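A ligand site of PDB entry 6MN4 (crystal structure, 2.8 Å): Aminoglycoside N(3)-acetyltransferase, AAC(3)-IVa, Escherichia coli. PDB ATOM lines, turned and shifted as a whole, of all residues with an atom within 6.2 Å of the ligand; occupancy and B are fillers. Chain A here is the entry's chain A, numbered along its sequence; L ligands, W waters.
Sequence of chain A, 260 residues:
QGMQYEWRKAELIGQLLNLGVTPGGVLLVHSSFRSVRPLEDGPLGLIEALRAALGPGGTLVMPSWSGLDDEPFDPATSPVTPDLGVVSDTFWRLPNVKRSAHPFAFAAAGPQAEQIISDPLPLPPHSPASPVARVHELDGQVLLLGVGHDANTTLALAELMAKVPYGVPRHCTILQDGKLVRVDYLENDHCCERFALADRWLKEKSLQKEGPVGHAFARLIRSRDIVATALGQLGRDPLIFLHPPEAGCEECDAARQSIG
Water W3 lies within hydrogen-bond range of OG1 of Thr 153 (2.5 Å) and N4 of the ligand (2.6 Å). Water W4 lies within hydrogen-bond range of N1 of the ligand (3.2 Å) and OE1 of Glu 251 (3.3 Å). Water W5 lies within hydrogen-bond range of a ring nitrogen (ND1) of His 171, the guanidinium group of Arg 182 and an oxygen (O9) of the ligand.
Trp 65 touches the ligand. Gly 67 touches the ligand (O to N2, 3.98 Å). Ten residues have an atom within 4 Å of the ligand: Trp 65, Gly 67, Asp 69, His 126, Arg 170, His 171, Glu 187, Asp 189, His 190 and Glu 251. The nearest printed residue that does not touch the ligand is Thr 153 (4.3 Å).
The guanidinium group (NH1) of Arg 170 lies within salt-bridge range of the side-chain carboxylate (OD2) of Asp 189 (2.4 Å). The backbone NH of Tyr 185 is in hydrogen-bond range of the backbone carbonyl oxygen of Arg 170 (2.9 Å). NE2 of His 171 sits close to O of Asp 69, 3.5 Å away. ND1 of His 171 is in hydrogen-bond range of NH2 of Arg 182 (2.9 Å). A ring nitrogen (ND1) of His 190 sits close to the backbone NH (N) of Cys 192 (3.2 Å).
N1 of the ligand is in salt-bridge range of OD2 of Asp 189. The backbone carbonyl oxygen (O) of His 190 is in hydrogen-bond range of a nitrogen (N1) of the ligand (3.3 Å). An oxygen (O11) of the ligand sits at hydrogen-bond distance from a ring nitrogen (NE2) of His 126 (2.7 Å). OD2 of Asp 69 lies within salt-bridge range of N2 of the ligand (3.5 Å). The guanidinium group (NH1) of Arg 170 sits at hydrogen-bond distance from an oxygen (O2) of the ligand, at 3.3 Å. O9 of the ligand is in hydrogen-bond range of ND1 of His 171 (2.9 Å). An oxygen (O11) of the ligand sits at hydrogen-bond distance from the side-chain carboxylate of Glu 187, at 3.0 Å. OE1 of Glu 251 is in salt-bridge range of N1 of the ligand.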
ATOM      1  N   TRP A  65     -23.197  17.531  25.682  1.00  0.00           N
ATOM      2  CA  TRP A  65     -23.317  18.802  24.983  1.00  0.00           C
ATOM      3  C   TRP A  65     -24.629  19.481  25.343  1.00  0.00           C
ATOM      4  O   TRP A  65     -25.575  18.868  25.852  1.00  0.00           O
ATOM      5  CB  TRP A  65     -23.206  18.614  23.478  1.00  0.00           C
ATOM      6  CG  TRP A  65     -24.181  17.651  22.875  1.00  0.00           C
ATOM      7  CD1 TRP A  65     -25.512  17.860  22.642  1.00  0.00           C
ATOM      8  CD2 TRP A  65     -23.906  16.314  22.422  1.00  0.00           C
ATOM      9  NE1 TRP A  65     -26.077  16.745  22.071  1.00  0.00           N
ATOM     10  CE2 TRP A  65     -25.116  15.781  21.933  1.00  0.00           C
ATOM     11  CE3 TRP A  65     -22.745  15.525  22.393  1.00  0.00           C
ATOM     12  CZ2 TRP A  65     -25.197  14.495  21.420  1.00  0.00           C
ATOM     13  CZ3 TRP A  65     -22.840  14.239  21.876  1.00  0.00           C
ATOM     14  CH2 TRP A  65     -24.053  13.739  21.392  1.00  0.00           C
ATOM     15  N   GLY A  67     -26.550  21.454  23.091  1.00  0.00           N
ATOM     16  CA  GLY A  67     -27.507  21.502  22.003  1.00  0.00           C
ATOM     17  C   GLY A  67     -27.976  22.887  21.634  1.00  0.00           C
ATOM     18  O   GLY A  67     -28.775  23.025  20.702  1.00  0.00           O
ATOM     19  N   LEU A  68     -27.506  23.921  22.322  1.00  0.00           N
ATOM     20  CA  LEU A  68     -27.887  25.291  22.026  1.00  0.00           C
ATOM     21  C   LEU A  68     -26.828  25.964  21.172  1.00  0.00           C
ATOM     22  O   LEU A  68     -25.624  25.802  21.396  1.00  0.00           O
ATOM     23  CB  LEU A  68     -28.106  26.088  23.310  1.00  0.00           C
ATOM     24  CG  LEU A  68     -28.863  25.358  24.404  1.00  0.00           C
ATOM     25  CD1 LEU A  68     -28.736  26.127  25.710  1.00  0.00           C
ATOM     26  CD2 LEU A  68     -30.324  25.155  24.008  1.00  0.00           C
ATOM     27  N   ASP A  69     -27.291  26.734  20.181  1.00  0.00           N
ATOM     28  CA  ASP A  69     -26.418  27.303  19.168  1.00  0.00           C
ATOM     29  C   ASP A  69     -26.194  28.807  19.333  1.00  0.00           C
ATOM     30  O   ASP A  69     -25.264  29.327  18.710  1.00  0.00           O
ATOM     31  CB  ASP A  69     -26.992  27.028  17.775  1.00  0.00           C
ATOM     32  CG  ASP A  69     -28.496  27.199  17.728  1.00  0.00           C
ATOM     33  OD1 ASP A  69     -29.103  27.458  18.788  1.00  0.00           O
ATOM     34  OD2 ASP A  69     -29.070  27.060  16.621  1.00  0.00           O
ATOM     35  N   ASP A  83     -32.395  15.807  25.068  1.00  0.00           N
ATOM     36  CA  ASP A  83     -32.442  14.582  24.286  1.00  0.00           C
ATOM     37  C   ASP A  83     -31.395  13.567  24.722  1.00  0.00           C
ATOM     38  O   ASP A  83     -31.443  12.424  24.261  1.00  0.00           O
ATOM     39  CB  ASP A  83     -32.271  14.899  22.806  1.00  0.00           C
ATOM     40  CG  ASP A  83     -33.003  13.909  21.910  1.00  0.00           C
ATOM     41  OD1 ASP A  83     -32.447  12.825  21.643  1.00  0.00           O
ATOM     42  OD2 ASP A  83     -34.142  14.223  21.491  1.00  0.00           O
ATOM     43  N   PHE A 104     -20.000  21.318  22.237  1.00  0.00           N
ATOM     44  CA  PHE A 104     -20.212  19.907  21.929  1.00  0.00           C
ATOM     45  C   PHE A 104     -19.482  19.000  22.906  1.00  0.00           C
ATOM     46  O   PHE A 104     -18.867  18.006  22.515  1.00  0.00           O
ATOM     47  CB  PHE A 104     -19.789  19.626  20.487  1.00  0.00           C
ATOM     48  CG  PHE A 104     -20.136  20.727  19.540  1.00  0.00           C
ATOM     49  CD1 PHE A 104     -21.450  20.952  19.166  1.00  0.00           C
ATOM     50  CD2 PHE A 104     -19.146  21.554  19.019  1.00  0.00           C
ATOM     51  CE1 PHE A 104     -21.780  21.982  18.292  1.00  0.00           C
ATOM     52  CE2 PHE A 104     -19.467  22.574  18.140  1.00  0.00           C
ATOM     53  CZ  PHE A 104     -20.785  22.790  17.781  1.00  0.00           C
ATOM     54  N   PRO A 125     -18.297  19.157  15.046  1.00  0.00           N
ATOM     55  CA  PRO A 125     -18.391  18.682  16.440  1.00  0.00           C
ATOM     56  C   PRO A 125     -17.837  17.285  16.672  1.00  0.00           C
ATOM     57  O   PRO A 125     -17.341  16.997  17.770  1.00  0.00           O
ATOM     58  CB  PRO A 125     -19.900  18.720  16.716  1.00  0.00           C
ATOM     59  CG  PRO A 125     -20.396  19.808  15.835  1.00  0.00           C
ATOM     60  CD  PRO A 125     -19.578  19.735  14.583  1.00  0.00           C
ATOM     61  N   HIS A 126     -17.890  16.402  15.675  1.00  0.00           N
ATOM     62  CA  HIS A 126     -17.412  15.038  15.841  1.00  0.00           C
ATOM     63  C   HIS A 126     -16.280  14.755  14.867  1.00  0.00           C
ATOM     64  O   HIS A 126     -16.278  13.732  14.174  1.00  0.00           O
ATOM     65  CB  HIS A 126     -18.571  14.066  15.672  1.00  0.00           C
ATOM     66  CG  HIS A 126     -19.776  14.444  16.472  1.00  0.00           C
ATOM     67  ND1 HIS A 126     -19.799  14.401  17.848  1.00  0.00           N
ATOM     68  CD2 HIS A 126     -21.002  14.895  16.087  1.00  0.00           C
ATOM     69  CE1 HIS A 126     -20.987  14.808  18.282  1.00  0.00           C
ATOM     70  NE2 HIS A 126     -21.731  15.100  17.231  1.00  0.00           N
ATOM     71  N   THR A 153     -22.888   8.160  18.278  1.00  0.00           N
ATOM     72  CA  THR A 153     -22.168   9.349  17.830  1.00  0.00           C
ATOM     73  C   THR A 153     -20.928   8.978  17.016  1.00  0.00           C
ATOM     74  O   THR A 153     -20.578   9.679  16.065  1.00  0.00           O
ATOM     75  CB  THR A 153     -21.806  10.212  19.041  1.00  0.00           C
ATOM     76  OG1 THR A 153     -23.002  10.740  19.615  1.00  0.00           O
ATOM     77  CG2 THR A 153     -20.906  11.358  18.621  1.00  0.00           C
ATOM     78  N   PRO A 169     -24.611  23.916   6.590  1.00  0.00           N
ATOM     79  CA  PRO A 169     -24.166  25.004   7.475  1.00  0.00           C
ATOM     80  C   PRO A 169     -24.862  24.955   8.828  1.00  0.00           C
ATOM     81  O   PRO A 169     -26.089  25.061   8.922  1.00  0.00           O
ATOM     82  CB  PRO A 169     -24.536  26.271   6.699  1.00  0.00           C
ATOM     83  CG  PRO A 169     -25.623  25.842   5.767  1.00  0.00           C
ATOM     84  CD  PRO A 169     -25.295  24.439   5.387  1.00  0.00           C
ATOM     85  N   ARG A 170     -24.057  24.789   9.879  1.00  0.00           N
ATOM     86  CA  ARG A 170     -24.525  24.835  11.248  1.00  0.00           C
ATOM     87  C   ARG A 170     -23.603  25.763  12.033  1.00  0.00           C
ATOM     88  O   ARG A 170     -22.475  26.031  11.619  1.00  0.00           O
ATOM     89  CB  ARG A 170     -24.555  23.441  11.879  1.00  0.00           C
ATOM     90  CG  ARG A 170     -25.515  22.472  11.191  1.00  0.00           C
ATOM     91  CD  ARG A 170     -26.962  22.824  11.475  1.00  0.00           C
ATOM     92  NE  ARG A 170     -27.838  22.579  10.329  1.00  0.00           N
ATOM     93  CZ  ARG A 170     -28.579  21.487  10.181  1.00  0.00           C
ATOM     94  NH1 ARG A 170     -28.538  20.532  11.102  1.00  0.00           N
ATOM     95  NH2 ARG A 170     -29.351  21.342   9.110  1.00  0.00           N
ATOM     96  N   HIS A 171     -24.090  26.279  13.161  1.00  0.00           N
ATOM     97  CA  HIS A 171     -23.324  27.253  13.914  1.00  0.00           C
ATOM     98  C   HIS A 171     -23.492  27.051  15.412  1.00  0.00           C
ATOM     99  O   HIS A 171     -24.433  26.401  15.871  1.00  0.00           O
ATOM    100  CB  HIS A 171     -23.713  28.684  13.542  1.00  0.00           C
ATOM    101  CG  HIS A 171     -24.948  29.172  14.212  1.00  0.00           C
ATOM    102  ND1 HIS A 171     -26.198  29.069  13.640  1.00  0.00           N
ATOM    103  CD2 HIS A 171     -25.144  29.779  15.416  1.00  0.00           C
ATOM    104  CE1 HIS A 171     -27.102  29.582  14.455  1.00  0.00           C
ATOM    105  NE2 HIS A 171     -26.484  30.021  15.534  1.00  0.00           N
ATOM    106  N   ARG A 182     -20.480  34.405  16.718  1.00  0.00           N
ATOM    107  CA  ARG A 182     -21.043  33.225  16.085  1.00  0.00           C
ATOM    108  C   ARG A 182     -19.950  32.528  15.273  1.00  0.00           C
ATOM    109  O   ARG A 182     -19.209  33.167  14.526  1.00  0.00           O
ATOM    110  CB  ARG A 182     -22.212  33.626  15.188  1.00  0.00           C
ATOM    111  CG  ARG A 182     -22.667  32.530  14.245  1.00  0.00           C
ATOM    112  CD  ARG A 182     -23.258  33.111  12.981  1.00  0.00           C
ATOM    113  NE  ARG A 182     -24.212  32.199  12.374  1.00  0.00           N
ATOM    114  CZ  ARG A 182     -25.533  32.304  12.503  1.00  0.00           C
ATOM    115  NH1 ARG A 182     -26.037  33.290  13.227  1.00  0.00           N
ATOM    116  NH2 ARG A 182     -26.330  31.432  11.912  1.00  0.00           N
ATOM    117  N   TYR A 185     -19.828  26.778  10.768  1.00  0.00           N
ATOM    118  CA  TYR A 185     -19.129  25.601  10.271  1.00  0.00           C
ATOM    119  C   TYR A 185     -20.082  24.814   9.376  1.00  0.00           C
ATOM    120  O   TYR A 185     -21.247  25.186   9.199  1.00  0.00           O
ATOM    121  CB  TYR A 185     -18.599  24.742  11.430  1.00  0.00           C
ATOM    122  CG  TYR A 185     -19.683  24.230  12.353  1.00  0.00           C
ATOM    123  CD1 TYR A 185     -20.245  22.978  12.169  1.00  0.00           C
ATOM    124  CD2 TYR A 185     -20.139  24.999  13.412  1.00  0.00           C
ATOM    125  CE1 TYR A 185     -21.231  22.504  13.018  1.00  0.00           C
ATOM    126  CE2 TYR A 185     -21.121  24.536  14.268  1.00  0.00           C
ATOM    127  CZ  TYR A 185     -21.669  23.283  14.067  1.00  0.00           C
ATOM    128  OH  TYR A 185     -22.659  22.810  14.902  1.00  0.00           O
ATOM    129  N   GLU A 187     -21.558  21.013   9.074  1.00  0.00           N
ATOM    130  CA  GLU A 187     -21.702  19.741   9.734  1.00  0.00           C
ATOM    131  C   GLU A 187     -22.313  18.707   8.799  1.00  0.00           C
ATOM    132  O   GLU A 187     -22.948  19.032   7.795  1.00  0.00           O
ATOM    133  CB  GLU A 187     -22.565  19.877  11.000  1.00  0.00           C
ATOM    134  CG  GLU A 187     -22.599  18.650  11.900  1.00  0.00           C
ATOM    135  CD  GLU A 187     -23.112  18.935  13.296  1.00  0.00           C
ATOM    136  OE1 GLU A 187     -23.929  19.865  13.456  1.00  0.00           O
ATOM    137  OE2 GLU A 187     -22.683  18.226  14.223  1.00  0.00           O
ATOM    138  N   ASP A 189     -24.842  16.413   9.432  1.00  0.00           N
ATOM    139  CA  ASP A 189     -25.970  15.861  10.159  1.00  0.00           C
ATOM    140  C   ASP A 189     -27.191  15.735   9.262  1.00  0.00           C
ATOM    141  O   ASP A 189     -27.287  16.360   8.204  1.00  0.00           O
ATOM    142  CB  ASP A 189     -26.316  16.701  11.411  1.00  0.00           C
ATOM    143  CG  ASP A 189     -26.644  18.144  11.079  1.00  0.00           C
ATOM    144  OD1 ASP A 189     -26.501  18.554   9.906  1.00  0.00           O
ATOM    145  OD2 ASP A 189     -27.048  18.865  12.017  1.00  0.00           O
ATOM    146  N   HIS A 190     -28.105  14.880   9.696  1.00  0.00           N
ATOM    147  CA  HIS A 190     -29.360  14.615   9.010  1.00  0.00           C
ATOM    148  C   HIS A 190     -30.323  14.010  10.030  1.00  0.00           C
ATOM    149  O   HIS A 190     -30.115  14.149  11.246  1.00  0.00           O
ATOM    150  CB  HIS A 190     -29.120  13.713   7.793  1.00  0.00           C
ATOM    151  CG  HIS A 190     -28.003  12.738   7.971  1.00  0.00           C
ATOM    152  ND1 HIS A 190     -28.096  11.641   8.802  1.00  0.00           N
ATOM    153  CD2 HIS A 190     -26.761  12.703   7.446  1.00  0.00           C
ATOM    154  CE1 HIS A 190     -26.962  10.968   8.769  1.00  0.00           C
ATOM    155  NE2 HIS A 190     -26.131  11.594   7.957  1.00  0.00           N
ATOM    156  N   CYS A 191     -31.353  13.332   9.544  1.00  0.00           N
ATOM    157  CA  CYS A 191     -32.309  12.699  10.441  1.00  0.00           C
ATOM    158  C   CYS A 191     -31.674  11.592  11.288  1.00  0.00           C
ATOM    159  O   CYS A 191     -32.196  11.269  12.353  1.00  0.00           O
ATOM    160  CB  CYS A 191     -33.486  12.139   9.639  1.00  0.00           C
ATOM    161  SG  CYS A 191     -33.107  10.740   8.583  1.00  0.00           S
ATOM    162  N   CYS A 192     -30.558  11.027  10.829  1.00  0.00           N
ATOM    163  CA  CYS A 192     -29.831   9.957  11.508  1.00  0.00           C
ATOM    164  C   CYS A 192     -30.654   8.682  11.657  1.00  0.00           C
ATOM    165  O   CYS A 192     -30.212   7.755  12.341  1.00  0.00           O
ATOM    166  CB  CYS A 192     -29.303  10.409  12.873  1.00  0.00           C
ATOM    167  SG  CYS A 192     -27.904  11.548  12.812  1.00  0.00           S
ATOM    168  N   GLU A 251     -34.795  16.722   6.271  1.00  0.00           N
ATOM    169  CA  GLU A 251     -33.429  16.831   6.790  1.00  0.00           C
ATOM    170  C   GLU A 251     -32.421  16.256   5.810  1.00  0.00           C
ATOM    171  O   GLU A 251     -31.394  16.871   5.525  1.00  0.00           O
ATOM    172  CB  GLU A 251     -33.340  16.131   8.144  1.00  0.00           C
ATOM    173  CG  GLU A 251     -32.370  16.774   9.122  1.00  0.00           C
ATOM    174  CD  GLU A 251     -32.751  16.531  10.572  1.00  0.00           C
ATOM    175  OE1 GLU A 251     -31.985  16.947  11.462  1.00  0.00           O
ATOM    176  OE2 GLU A 251     -33.817  15.925  10.816  1.00  0.00           O
HETATM  177  C1  LIG L   1     -29.632  17.573  15.682  1.00  0.00           C
HETATM  178  C2  LIG L   1     -30.350  17.628  14.330  1.00  0.00           C
HETATM  179  C3  LIG L   1     -30.173  18.978  13.624  1.00  0.00           C
HETATM  180  C4  LIG L   1     -30.447  20.141  14.524  1.00  0.00           C
HETATM  181  C5  LIG L   1     -29.650  20.017  15.855  1.00  0.00           C
HETATM  182  C6  LIG L   1     -29.848  21.212  16.700  1.00  0.00           C
HETATM  183  C7  LIG L   1     -29.305  22.435  15.930  1.00  0.00           C
HETATM  184  C8  LIG L   1     -30.133  22.682  14.648  1.00  0.00           C
HETATM  185  C9  LIG L   1     -30.502  24.236  17.061  1.00  0.00           C
HETATM  186  O1  LIG L   1     -30.015  18.762  16.566  1.00  0.00           O
HETATM  187  O2  LIG L   1     -30.226  21.443  13.786  1.00  0.00           O
HETATM  188  N1  LIG L   1     -29.796  16.579  13.468  1.00  0.00           N
HETATM  189  N2  LIG L   1     -29.207  23.610  16.788  1.00  0.00           N
HETATM  190  O3  LIG L   1     -31.257  21.330  16.930  1.00  0.00           O
HETATM  191  O4  LIG L   1     -29.504  23.596  13.875  1.00  0.00           O
HETATM  192  O5  LIG L   1     -28.298  17.651  15.462  1.00  0.00           O
HETATM  193  C10 LIG L   1     -30.297  24.655  13.524  1.00  0.00           C
HETATM  194  C11 LIG L   1     -31.699  24.266  13.026  1.00  0.00           C
HETATM  195  C12 LIG L   1     -32.465  25.432  12.532  1.00  0.00           C
HETATM  196  C13 LIG L   1     -31.745  26.733  12.681  1.00  0.00           C
HETATM  197  C14 LIG L   1     -30.287  26.674  12.142  1.00  0.00           C
HETATM  198  C15 LIG L   1     -29.508  27.785  12.746  1.00  0.00           C
HETATM  199  O6  LIG L   1     -29.588  25.437  12.470  1.00  0.00           O
HETATM  200  N3  LIG L   1     -32.487  27.786  11.958  1.00  0.00           N
HETATM  201  O7  LIG L   1     -31.585  23.318  11.946  1.00  0.00           O
HETATM  202  O8  LIG L   1     -33.734  25.508  13.260  1.00  0.00           O
HETATM  203  O9  LIG L   1     -28.347  27.224  13.296  1.00  0.00           O
HETATM  204  C16 LIG L   1     -27.500  16.621  16.103  1.00  0.00           C
HETATM  205  C17 LIG L   1     -26.099  17.211  16.129  1.00  0.00           C
HETATM  206  C18 LIG L   1     -25.103  16.154  16.634  1.00  0.00           C
HETATM  207  C19 LIG L   1     -25.382  15.773  18.069  1.00  0.00           C
HETATM  208  C20 LIG L   1     -26.871  15.755  18.493  1.00  0.00           C
HETATM  209  C21 LIG L   1     -27.973  16.224  17.498  1.00  0.00           C
HETATM  210  N4  LIG L   1     -24.819  14.439  18.287  1.00  0.00           N
HETATM  211  N5  LIG L   1     -28.920  15.108  17.413  1.00  0.00           N
HETATM  212  O10 LIG L   1     -25.752  17.632  14.839  1.00  0.00           O
HETATM  213  O11 LIG L   1     -23.809  16.690  16.564  1.00  0.00           O
HETATM  214  O   HOH W   1     -32.585  26.657  16.977  1.00  0.00           O
HETATM  215  O   HOH W   2     -30.970  13.837  15.712  1.00  0.00           O
HETATM  216  O   HOH W   3     -24.460  11.872  17.947  1.00  0.00           O
HETATM  217  O   HOH W   4     -32.605  15.347  14.283  1.00  0.00           O
HETATM  218  O   HOH W   5     -26.595  28.364  10.564  1.00  0.00           O
